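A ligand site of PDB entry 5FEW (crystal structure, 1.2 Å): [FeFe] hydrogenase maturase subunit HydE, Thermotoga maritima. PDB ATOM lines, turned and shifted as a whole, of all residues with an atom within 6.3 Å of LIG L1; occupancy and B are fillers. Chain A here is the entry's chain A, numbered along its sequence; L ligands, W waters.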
ATOM      1  N   VAL A  72       3.588   8.185 -14.077  1.00  0.00           N
ATOM      2  CA  VAL A  72       2.821   8.129 -15.347  1.00  0.00           C
ATOM      3  C   VAL A  72       3.461   9.089 -16.315  1.00  0.00           C
ATOM      4  O   VAL A  72       3.726  10.240 -15.975  1.00  0.00           O
ATOM      5  CB  VAL A  72       1.367   8.471 -15.096  1.00  0.00           C
ATOM      6  CG1 VAL A  72       0.572   8.614 -16.405  1.00  0.00           C
ATOM      7  CG2 VAL A  72       0.730   7.425 -14.175  1.00  0.00           C
ATOM      8  N   CYS A  73       3.670   8.656 -17.559  1.00  0.00           N
ATOM      9  CA  CYS A  73       4.176   9.564 -18.571  1.00  0.00           C
ATOM     10  C   CYS A  73       3.544   9.291 -19.923  1.00  0.00           C
ATOM     11  O   CYS A  73       3.358   8.169 -20.342  1.00  0.00           O
ATOM     12  CB  CYS A  73       5.712   9.455 -18.728  1.00  0.00           C
ATOM     13  SG  CYS A  73       6.346  10.918 -19.641  1.00  0.00           S
ATOM     14  N   ARG A  74       3.228  10.402 -20.577  1.00  0.00           N
ATOM     15  CA  ARG A  74       2.674  10.390 -21.962  1.00  0.00           C
ATOM     16  C   ARG A  74       3.754  10.349 -23.041  1.00  0.00           C
ATOM     17  O   ARG A  74       3.416  10.067 -24.217  1.00  0.00           O
ATOM     18  CB  ARG A  74       1.802  11.606 -22.188  1.00  0.00           C
ATOM     19  CG  ARG A  74       2.586  12.923 -22.242  1.00  0.00           C
ATOM     20  CD  ARG A  74       1.721  14.123 -22.321  1.00  0.00           C
ATOM     21  NE  ARG A  74       2.467  15.336 -22.291  1.00  0.00           N
ATOM     22  CZ  ARG A  74       2.044  16.506 -22.648  1.00  0.00           C
ATOM     23  NH1 ARG A  74       0.810  16.664 -23.108  1.00  0.00           N
ATOM     24  NH2 ARG A  74       2.837  17.549 -22.615  1.00  0.00           N
ATOM     25  N   LYS A  75       5.016  10.614 -22.702  1.00  0.00           N
ATOM     26  CA  LYS A  75       6.106  10.628 -23.676  1.00  0.00           C
ATOM     27  C   LYS A  75       6.810   9.275 -23.694  1.00  0.00           C
ATOM     28  O   LYS A  75       6.577   8.402 -22.866  1.00  0.00           O
ATOM     29  CB  LYS A  75       7.060  11.764 -23.380  1.00  0.00           C
ATOM     30  CG  LYS A  75       6.549  13.134 -23.899  1.00  0.00           C
ATOM     31  CD  LYS A  75       7.574  14.228 -23.771  1.00  0.00           C
ATOM     32  CE  LYS A  75       7.288  15.483 -24.525  1.00  0.00           C
ATOM     33  NZ  LYS A  75       5.937  16.012 -24.317  1.00  0.00           N
ATOM     34  N   ASN A  76       7.696   9.114 -24.683  1.00  0.00           N
ATOM     35  CA  ASN A  76       8.319   7.834 -25.013  1.00  0.00           C
ATOM     36  C   ASN A  76       9.822   7.960 -25.202  1.00  0.00           C
ATOM     37  O   ASN A  76      10.420   7.278 -26.034  1.00  0.00           O
ATOM     38  CB  ASN A  76       7.660   7.214 -26.248  1.00  0.00           C
ATOM     39  CG  ASN A  76       7.620   5.748 -26.226  1.00  0.00           C
ATOM     40  OD1 ASN A  76       7.636   5.065 -25.219  1.00  0.00           O
ATOM     41  ND2 ASN A  76       7.482   5.161 -27.455  1.00  0.00           N
ATOM     42  N   CYS A  77      10.446   8.806 -24.407  1.00  0.00           N
ATOM     43  CA  CYS A  77      11.872   9.041 -24.535  1.00  0.00           C
ATOM     44  C   CYS A  77      12.631   7.736 -24.520  1.00  0.00           C
ATOM     45  O   CYS A  77      12.375   6.867 -23.685  1.00  0.00           O
ATOM     46  CB  CYS A  77      12.406  10.004 -23.429  1.00  0.00           C
ATOM     47  SG  CYS A  77      11.488  11.555 -23.340  1.00  0.00           S
ATOM     48  N   TYR A  79      15.543   6.695 -23.697  1.00  0.00           N
ATOM     49  CA  TYR A  79      16.472   6.392 -22.591  1.00  0.00           C
ATOM     50  C   TYR A  79      15.769   6.063 -21.290  1.00  0.00           C
ATOM     51  O   TYR A  79      16.403   5.531 -20.338  1.00  0.00           O
ATOM     52  CB  TYR A  79      17.426   7.512 -22.339  1.00  0.00           C
ATOM     53  CG  TYR A  79      16.834   8.893 -22.380  1.00  0.00           C
ATOM     54  CD1 TYR A  79      16.163   9.441 -21.266  1.00  0.00           C
ATOM     55  CD2 TYR A  79      16.866   9.710 -23.498  1.00  0.00           C
ATOM     56  CE1 TYR A  79      15.600  10.677 -21.308  1.00  0.00           C
ATOM     57  CE2 TYR A  79      16.260  10.945 -23.542  1.00  0.00           C
ATOM     58  CZ  TYR A  79      15.629  11.436 -22.437  1.00  0.00           C
ATOM     59  OH  TYR A  79      15.043  12.684 -22.502  1.00  0.00           O
ATOM     60  N   CYS A  80      14.467   6.428 -21.147  1.00  0.00           N
ATOM     61  CA  CYS A  80      13.843   6.586 -19.847  1.00  0.00           C
ATOM     62  C   CYS A  80      12.993   5.362 -19.466  1.00  0.00           C
ATOM     63  O   CYS A  80      12.071   4.960 -20.230  1.00  0.00           O
ATOM     64  CB  CYS A  80      12.969   7.813 -19.843  1.00  0.00           C
ATOM     65  SG  CYS A  80      12.217   8.134 -18.230  1.00  0.00           S
ATOM     66  N   GLY A  81      13.201   4.809 -18.260  1.00  0.00           N
ATOM     67  CA  GLY A  81      12.380   3.749 -17.779  1.00  0.00           C
ATOM     68  C   GLY A  81      10.900   4.044 -17.561  1.00  0.00           C
ATOM     69  O   GLY A  81      10.095   3.115 -17.463  1.00  0.00           O
ATOM     70  N   LEU A  82      10.510   5.323 -17.541  1.00  0.00           N
ATOM     71  CA  LEU A  82       9.125   5.700 -17.380  1.00  0.00           C
ATOM     72  C   LEU A  82       8.408   5.876 -18.731  1.00  0.00           C
ATOM     73  O   LEU A  82       7.242   6.166 -18.768  1.00  0.00           O
ATOM     74  CB  LEU A  82       8.931   7.001 -16.570  1.00  0.00           C
ATOM     75  CG  LEU A  82       9.554   6.969 -15.190  1.00  0.00           C
ATOM     76  CD1 LEU A  82       9.115   8.258 -14.458  1.00  0.00           C
ATOM     77  CD2 LEU A  82       9.484   5.787 -14.380  1.00  0.00           C
ATOM     78  N   ARG A  83       9.130   5.650 -19.828  1.00  0.00           N
ATOM     79  CA  ARG A  83       8.524   5.890 -21.158  1.00  0.00           C
ATOM     80  C   ARG A  83       7.211   5.126 -21.282  1.00  0.00           C
ATOM     81  O   ARG A  83       7.034   4.041 -20.756  1.00  0.00           O
ATOM     82  CB  ARG A  83       9.516   5.485 -22.241  1.00  0.00           C
ATOM     83  CG  ARG A  83       9.853   3.991 -22.313  1.00  0.00           C
ATOM     84  CD  ARG A  83      11.081   3.720 -23.099  1.00  0.00           C
ATOM     85  NE  ARG A  83      11.071   4.355 -24.402  1.00  0.00           N
ATOM     86  CZ  ARG A  83      10.605   3.772 -25.535  1.00  0.00           C
ATOM     87  NH1 ARG A  83      10.193   2.523 -25.513  1.00  0.00           N
ATOM     88  NH2 ARG A  83      10.610   4.467 -26.623  1.00  0.00           N
ATOM     89  N   ARG A  84       6.305   5.731 -22.071  1.00  0.00           N
ATOM     90  CA  ARG A  84       4.945   5.136 -22.137  1.00  0.00           C
ATOM     91  C   ARG A  84       4.901   3.722 -22.606  1.00  0.00           C
ATOM     92  O   ARG A  84       4.022   2.950 -22.182  1.00  0.00           O
ATOM     93  CB  ARG A  84       3.972   5.939 -22.894  1.00  0.00           C
ATOM     94  CG  ARG A  84       4.244   6.099 -24.332  1.00  0.00           C
ATOM     95  CD  ARG A  84       3.038   6.814 -25.100  1.00  0.00           C
ATOM     96  NE  ARG A  84       3.410   6.694 -26.465  1.00  0.00           N
ATOM     97  CZ  ARG A  84       4.060   7.621 -27.152  1.00  0.00           C
ATOM     98  NH1 ARG A  84       4.363   8.807 -26.640  1.00  0.00           N
ATOM     99  NH2 ARG A  84       4.501   7.326 -28.358  1.00  0.00           N
ATOM    100  N   SER A 118       7.728  14.575 -11.756  1.00  0.00           N
ATOM    101  CA  SER A 118       6.898  13.477 -12.219  1.00  0.00           C
ATOM    102  C   SER A 118       7.240  13.172 -13.660  1.00  0.00           C
ATOM    103  O   SER A 118       7.868  13.966 -14.370  1.00  0.00           O
ATOM    104  CB  SER A 118       5.420  13.857 -12.096  1.00  0.00           C
ATOM    105  OG  SER A 118       5.065  14.985 -12.858  1.00  0.00           O
ATOM    106  N   GLY A 119       6.704  12.026 -14.124  1.00  0.00           N
ATOM    107  CA  GLY A 119       6.491  11.867 -15.562  1.00  0.00           C
ATOM    108  C   GLY A 119       5.570  12.962 -16.071  1.00  0.00           C
ATOM    109  O   GLY A 119       4.895  13.662 -15.275  1.00  0.00           O
ATOM    110  N   GLU A 120       5.449  13.113 -17.392  1.00  0.00           N
ATOM    111  CA  GLU A 120       4.461  14.008 -17.949  1.00  0.00           C
ATOM    112  C   GLU A 120       3.083  13.362 -17.836  1.00  0.00           C
ATOM    113  O   GLU A 120       2.568  12.740 -18.782  1.00  0.00           O
ATOM    114  CB  GLU A 120       4.758  14.398 -19.394  1.00  0.00           C
ATOM    115  CG  GLU A 120       5.996  15.269 -19.528  1.00  0.00           C
ATOM    116  CD  GLU A 120       6.123  15.924 -20.874  1.00  0.00           C
ATOM    117  OE1 GLU A 120       5.180  15.805 -21.700  1.00  0.00           O
ATOM    118  OE2 GLU A 120       7.165  16.574 -21.142  1.00  0.00           O
ATOM    119  N   GLY A 148       8.191  18.524 -16.922  1.00  0.00           N
ATOM    120  CA  GLY A 148       8.281  18.360 -18.381  1.00  0.00           C
ATOM    121  C   GLY A 148       7.765  19.568 -19.134  1.00  0.00           C
ATOM    122  O   GLY A 148       7.710  20.704 -18.647  1.00  0.00           O
ATOM    123  N   GLU A 171      18.791  18.037 -22.114  1.00  0.00           N
ATOM    124  CA  GLU A 171      19.096  16.664 -22.436  1.00  0.00           C
ATOM    125  C   GLU A 171      20.308  16.498 -23.415  1.00  0.00           C
ATOM    126  O   GLU A 171      21.293  15.833 -23.085  1.00  0.00           O
ATOM    127  CB  GLU A 171      17.844  15.910 -22.972  1.00  0.00           C
ATOM    128  CG  GLU A 171      16.585  16.025 -22.094  1.00  0.00           C
ATOM    129  CD  GLU A 171      16.724  15.524 -20.691  1.00  0.00           C
ATOM    130  OE1 GLU A 171      17.832  15.087 -20.257  1.00  0.00           O
ATOM    131  OE2 GLU A 171      15.672  15.561 -19.984  1.00  0.00           O
ATOM    132  N   ARG A 182      13.954  11.614 -28.341  1.00  0.00           N
ATOM    133  CA  ARG A 182      12.775  12.163 -27.706  1.00  0.00           C
ATOM    134  C   ARG A 182      11.738  12.381 -28.855  1.00  0.00           C
ATOM    135  O   ARG A 182      11.463  13.528 -29.265  1.00  0.00           O
ATOM    136  CB  ARG A 182      13.098  13.439 -26.960  1.00  0.00           C
ATOM    137  CG  ARG A 182      14.229  13.245 -25.982  1.00  0.00           C
ATOM    138  CD  ARG A 182      14.486  14.412 -25.068  1.00  0.00           C
ATOM    139  NE  ARG A 182      13.366  14.521 -24.129  1.00  0.00           N
ATOM    140  CZ  ARG A 182      12.426  15.452 -24.132  1.00  0.00           C
ATOM    141  NH1 ARG A 182      12.513  16.548 -24.831  1.00  0.00           N
ATOM    142  NH2 ARG A 182      11.336  15.285 -23.350  1.00  0.00           N
ATOM    143  N   ARG A 190      11.892  22.178 -26.613  1.00  0.00           N
ATOM    144  CA  ARG A 190      12.515  22.187 -25.280  1.00  0.00           C
ATOM    145  C   ARG A 190      13.086  23.545 -24.936  1.00  0.00           C
ATOM    146  O   ARG A 190      12.894  24.079 -23.844  1.00  0.00           O
ATOM    147  CB  ARG A 190      13.605  21.082 -25.247  1.00  0.00           C
ATOM    148  CG  ARG A 190      14.097  20.686 -23.872  1.00  0.00           C
ATOM    149  CD  ARG A 190      13.128  19.799 -23.243  1.00  0.00           C
ATOM    150  NE  ARG A 190      13.609  19.084 -22.024  1.00  0.00           N
ATOM    151  CZ  ARG A 190      12.869  18.289 -21.242  1.00  0.00           C
ATOM    152  NH1 ARG A 190      11.635  18.029 -21.604  1.00  0.00           N
ATOM    153  NH2 ARG A 190      13.385  17.799 -20.136  1.00  0.00           N
ATOM    154  N   TYR A 313       9.867   4.508  -9.217  1.00  0.00           N
ATOM    155  CA  TYR A 313      10.267   5.664  -9.980  1.00  0.00           C
ATOM    156  C   TYR A 313      11.684   5.411 -10.441  1.00  0.00           C
ATOM    157  O   TYR A 313      12.625   5.939  -9.861  1.00  0.00           O
ATOM    158  CB  TYR A 313      10.139   6.932  -9.181  1.00  0.00           C
ATOM    159  CG  TYR A 313      10.171   8.189 -10.042  1.00  0.00           C
ATOM    160  CD1 TYR A 313       8.982   8.752 -10.548  1.00  0.00           C
ATOM    161  CD2 TYR A 313      11.319   8.836 -10.328  1.00  0.00           C
ATOM    162  CE1 TYR A 313       8.949   9.933 -11.258  1.00  0.00           C
ATOM    163  CE2 TYR A 313      11.338  10.031 -11.004  1.00  0.00           C
ATOM    164  CZ  TYR A 313      10.167  10.572 -11.469  1.00  0.00           C
ATOM    165  OH  TYR A 313      10.164  11.803 -12.036  1.00  0.00           O
ATOM    166  N   LEU A 315      13.913   5.739 -13.401  1.00  0.00           N
ATOM    167  CA  LEU A 315      14.328   6.239 -14.702  1.00  0.00           C
ATOM    168  C   LEU A 315      15.410   5.407 -15.299  1.00  0.00           C
ATOM    169  O   LEU A 315      15.466   5.226 -16.494  1.00  0.00           O
ATOM    170  CB  LEU A 315      14.834   7.736 -14.583  1.00  0.00           C
ATOM    171  CG  LEU A 315      13.939   8.733 -13.839  1.00  0.00           C
ATOM    172  CD1 LEU A 315      14.678  10.023 -13.685  1.00  0.00           C
ATOM    173  CD2 LEU A 315      12.708   8.834 -14.402  1.00  0.00           C
HETATM  174 FE1  LIG L   1      10.992   9.948 -18.899  1.00  0.00          FE
HETATM  175 FE2  LIG L   1       8.603  10.944 -19.572  1.00  0.00          FE
HETATM  176 FE3  LIG L   1      10.776  11.480 -21.109  1.00  0.00          FE
HETATM  177 FE4  LIG L   1      10.652  12.746 -18.455  1.00  0.00          FE
HETATM  178  S1  LIG L   1       9.244  13.007 -20.433  1.00  0.00           S
HETATM  179  S2  LIG L   1      12.450  11.621 -19.527  1.00  0.00           S
HETATM  180  S3  LIG L   1       9.529  10.860 -17.483  1.00  0.00           S
HETATM  181  S4  LIG L   1       9.752   9.430 -20.789  1.00  0.00           S
HETATM  182  N1  LG2 L   2       9.475  14.196 -17.211  1.00  0.00           N
HETATM  183  C1  LG2 L   2      10.209  15.404 -16.820  1.00  0.00           C
HETATM  184  C2  LG2 L   2      11.239  15.676 -17.857  1.00  0.00           C
HETATM  185  O1  LG2 L   2      11.790  16.825 -17.836  1.00  0.00           O
HETATM  186  C3  LG2 L   2      10.888  15.307 -15.365  1.00  0.00           C
HETATM  187  C4  LG2 L   2      12.217  14.501 -15.380  1.00  0.00           C
HETATM  188  S1  LG2 L   2      12.217  12.852 -16.110  1.00  0.00           S
HETATM  189  C5  LG2 L   2      11.232  12.037 -14.819  1.00  0.00           C
HETATM  190  O2  LG2 L   2      11.518  14.755 -18.678  1.00  0.00           O
HETATM  191  N1  LG3 L   3      19.932   7.592 -17.348  1.00  0.00           N
HETATM  192  C1  LG3 L   3      17.801   8.529 -17.623  1.00  0.00           C
HETATM  193  C2  LG3 L   3      16.267   9.960 -17.639  1.00  0.00           C
HETATM  194  C3  LG3 L   3      20.258   8.732 -16.677  1.00  0.00           C
HETATM  195  C4  LG3 L   3      18.681   7.454 -17.742  1.00  0.00           C
HETATM  196  N2  LG3 L   3      19.492   9.818 -16.543  1.00  0.00           N
HETATM  197  C5  LG3 L   3      18.290   9.653 -17.032  1.00  0.00           C
HETATM  198  O1  LG3 L   3      18.352  10.713 -10.707  1.00  0.00           O
HETATM  199  C6  LG3 L   3      18.921  11.821 -10.963  1.00  0.00           C
HETATM  200  O2  LG3 L   3      20.110  11.883 -11.184  1.00  0.00           O
HETATM  201  C7  LG3 L   3      17.980  12.956 -11.148  1.00  0.00           C
HETATM  202  N3  LG3 L   3      18.776  14.193 -10.794  1.00  0.00           N
HETATM  203  C8  LG3 L   3      17.299  12.914 -12.468  1.00  0.00           C
HETATM  204  S1  LG3 L   3      16.414  14.429 -12.886  1.00  0.00           S
HETATM  205  C9  LG3 L   3      15.570  13.998 -14.459  1.00  0.00           C
HETATM  206  C10 LG3 L   3      16.555  13.746 -15.600  1.00  0.00           C
HETATM  207  O3  LG3 L   3      17.021  12.319 -15.479  1.00  0.00           O
HETATM  208  C11 LG3 L   3      15.982  13.693 -17.013  1.00  0.00           C
HETATM  209  O4  LG3 L   3      15.802  15.092 -17.467  1.00  0.00           O
HETATM  210  C12 LG3 L   3      17.053  12.965 -17.827  1.00  0.00           C
HETATM  211  O5  LG3 L   3      18.181  13.823 -18.060  1.00  0.00           O
HETATM  212  C13 LG3 L   3      17.578  11.973 -16.703  1.00  0.00           C
HETATM  213  N4  LG3 L   3      17.310  10.554 -17.028  1.00  0.00           N
HETATM  214  N5  LG3 L   3      16.483   8.673 -17.975  1.00  0.00           N
HETATM  215  N6  LG3 L   3      18.343   6.290 -18.370  1.00  0.00           N
HETATM  216  O   HOH W   1       9.763  16.225 -20.639  1.00  0.00           O
HETATM  217  O   HOH W   2      13.450  14.290 -21.032  1.00  0.00           O
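An iron atom (FE2) of LIG L1 is bound by the side-chain sulfur (SG) of Cys 73 (2.3 Å). SG of Cys 77 is bound to FE3 of LIG L1, 2.3 Å away. SG of Cys 80 is bound to FE1 of LIG L1 (2.3 Å). The backbone carbonyl oxygen (O) of Ser 118 lies close to a nitrogen (N1) of LG2 L2, 3.3 Å away. NH2 of Arg 190 lies within salt-bridge range of O1 of LG2 L2. The backbone NH of Cys 77 sits close to a sulfur (S4) of LIG L1. The backbone carbonyl oxygen of Tyr 79 lies within hydrogen-bond range of a nitrogen (N6) of LG3 L3 (2.9 Å). An oxygen (O5) of LG3 L3 sits at hydrogen-bond distance from the side-chain carboxylate of Glu 171, 2.6 Å away.
An oxygen (O2) of LG2 L2 is bound to an iron atom (FE4) of LIG L1.
SG of Cys 80 sits close to N of Leu 82, 3.4 Å away. The side-chain amino group (NZ) of Lys 75 lies within salt-bridge range of the side-chain carboxylate (OE1) of Glu 120 (2.7 Å). SG of Cys 73 sits close to N of Lys 75. The backbone carbonyl oxygen (O) of Cys 77 lies within hydrogen-bond range of the guanidinium group (NE) of Arg 83, 2.9 Å away. NH2 of Arg 83 lies within hydrogen-bond range of O of Asn 76 (2.9 Å). The backbone carbonyl oxygen (O) of Lys 75 is in hydrogen-bond range of the backbone NH (N) of Arg 84 (2.8 Å). The guanidinium group (NE) of Arg 182 lies close to the side-chain sulfur (SG) of Cys 77 (3.6 Å). The backbone NH (N) of Glu 120 lies close to the side-chain sulfur (SG) of Cys 73 (3.3 Å).
CB of Lys 75 touches S1 of LIG L1, at 3.9 Å. CE1 of Tyr 79 touches S2 of LIG L1 (3.7 Å). CA of Arg 83 touches S4 of LIG L1, at 3.8 Å. Gly 119 touches LIG L1 (CA to S3, 3.7 Å). The nearest printed residue that does not touch LIG L1 is Leu 82 (4.01 Å).
Water W2 lies within hydrogen-bond range of the side-chain hydroxyl (OH) of Tyr 79, the side-chain carboxylate (OE2) of Glu 171, the guanidinium group (NE) of Arg 182 and a sulfur (S2) of LIG L1. Water W1 lies within hydrogen-bond range of the side-chain carboxylate (OE2) of Glu 120, the guanidinium group (NH1) of Arg 190, a sulfur (S1) of LIG L1 and the guanidinium group (NH2) of Arg 182.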
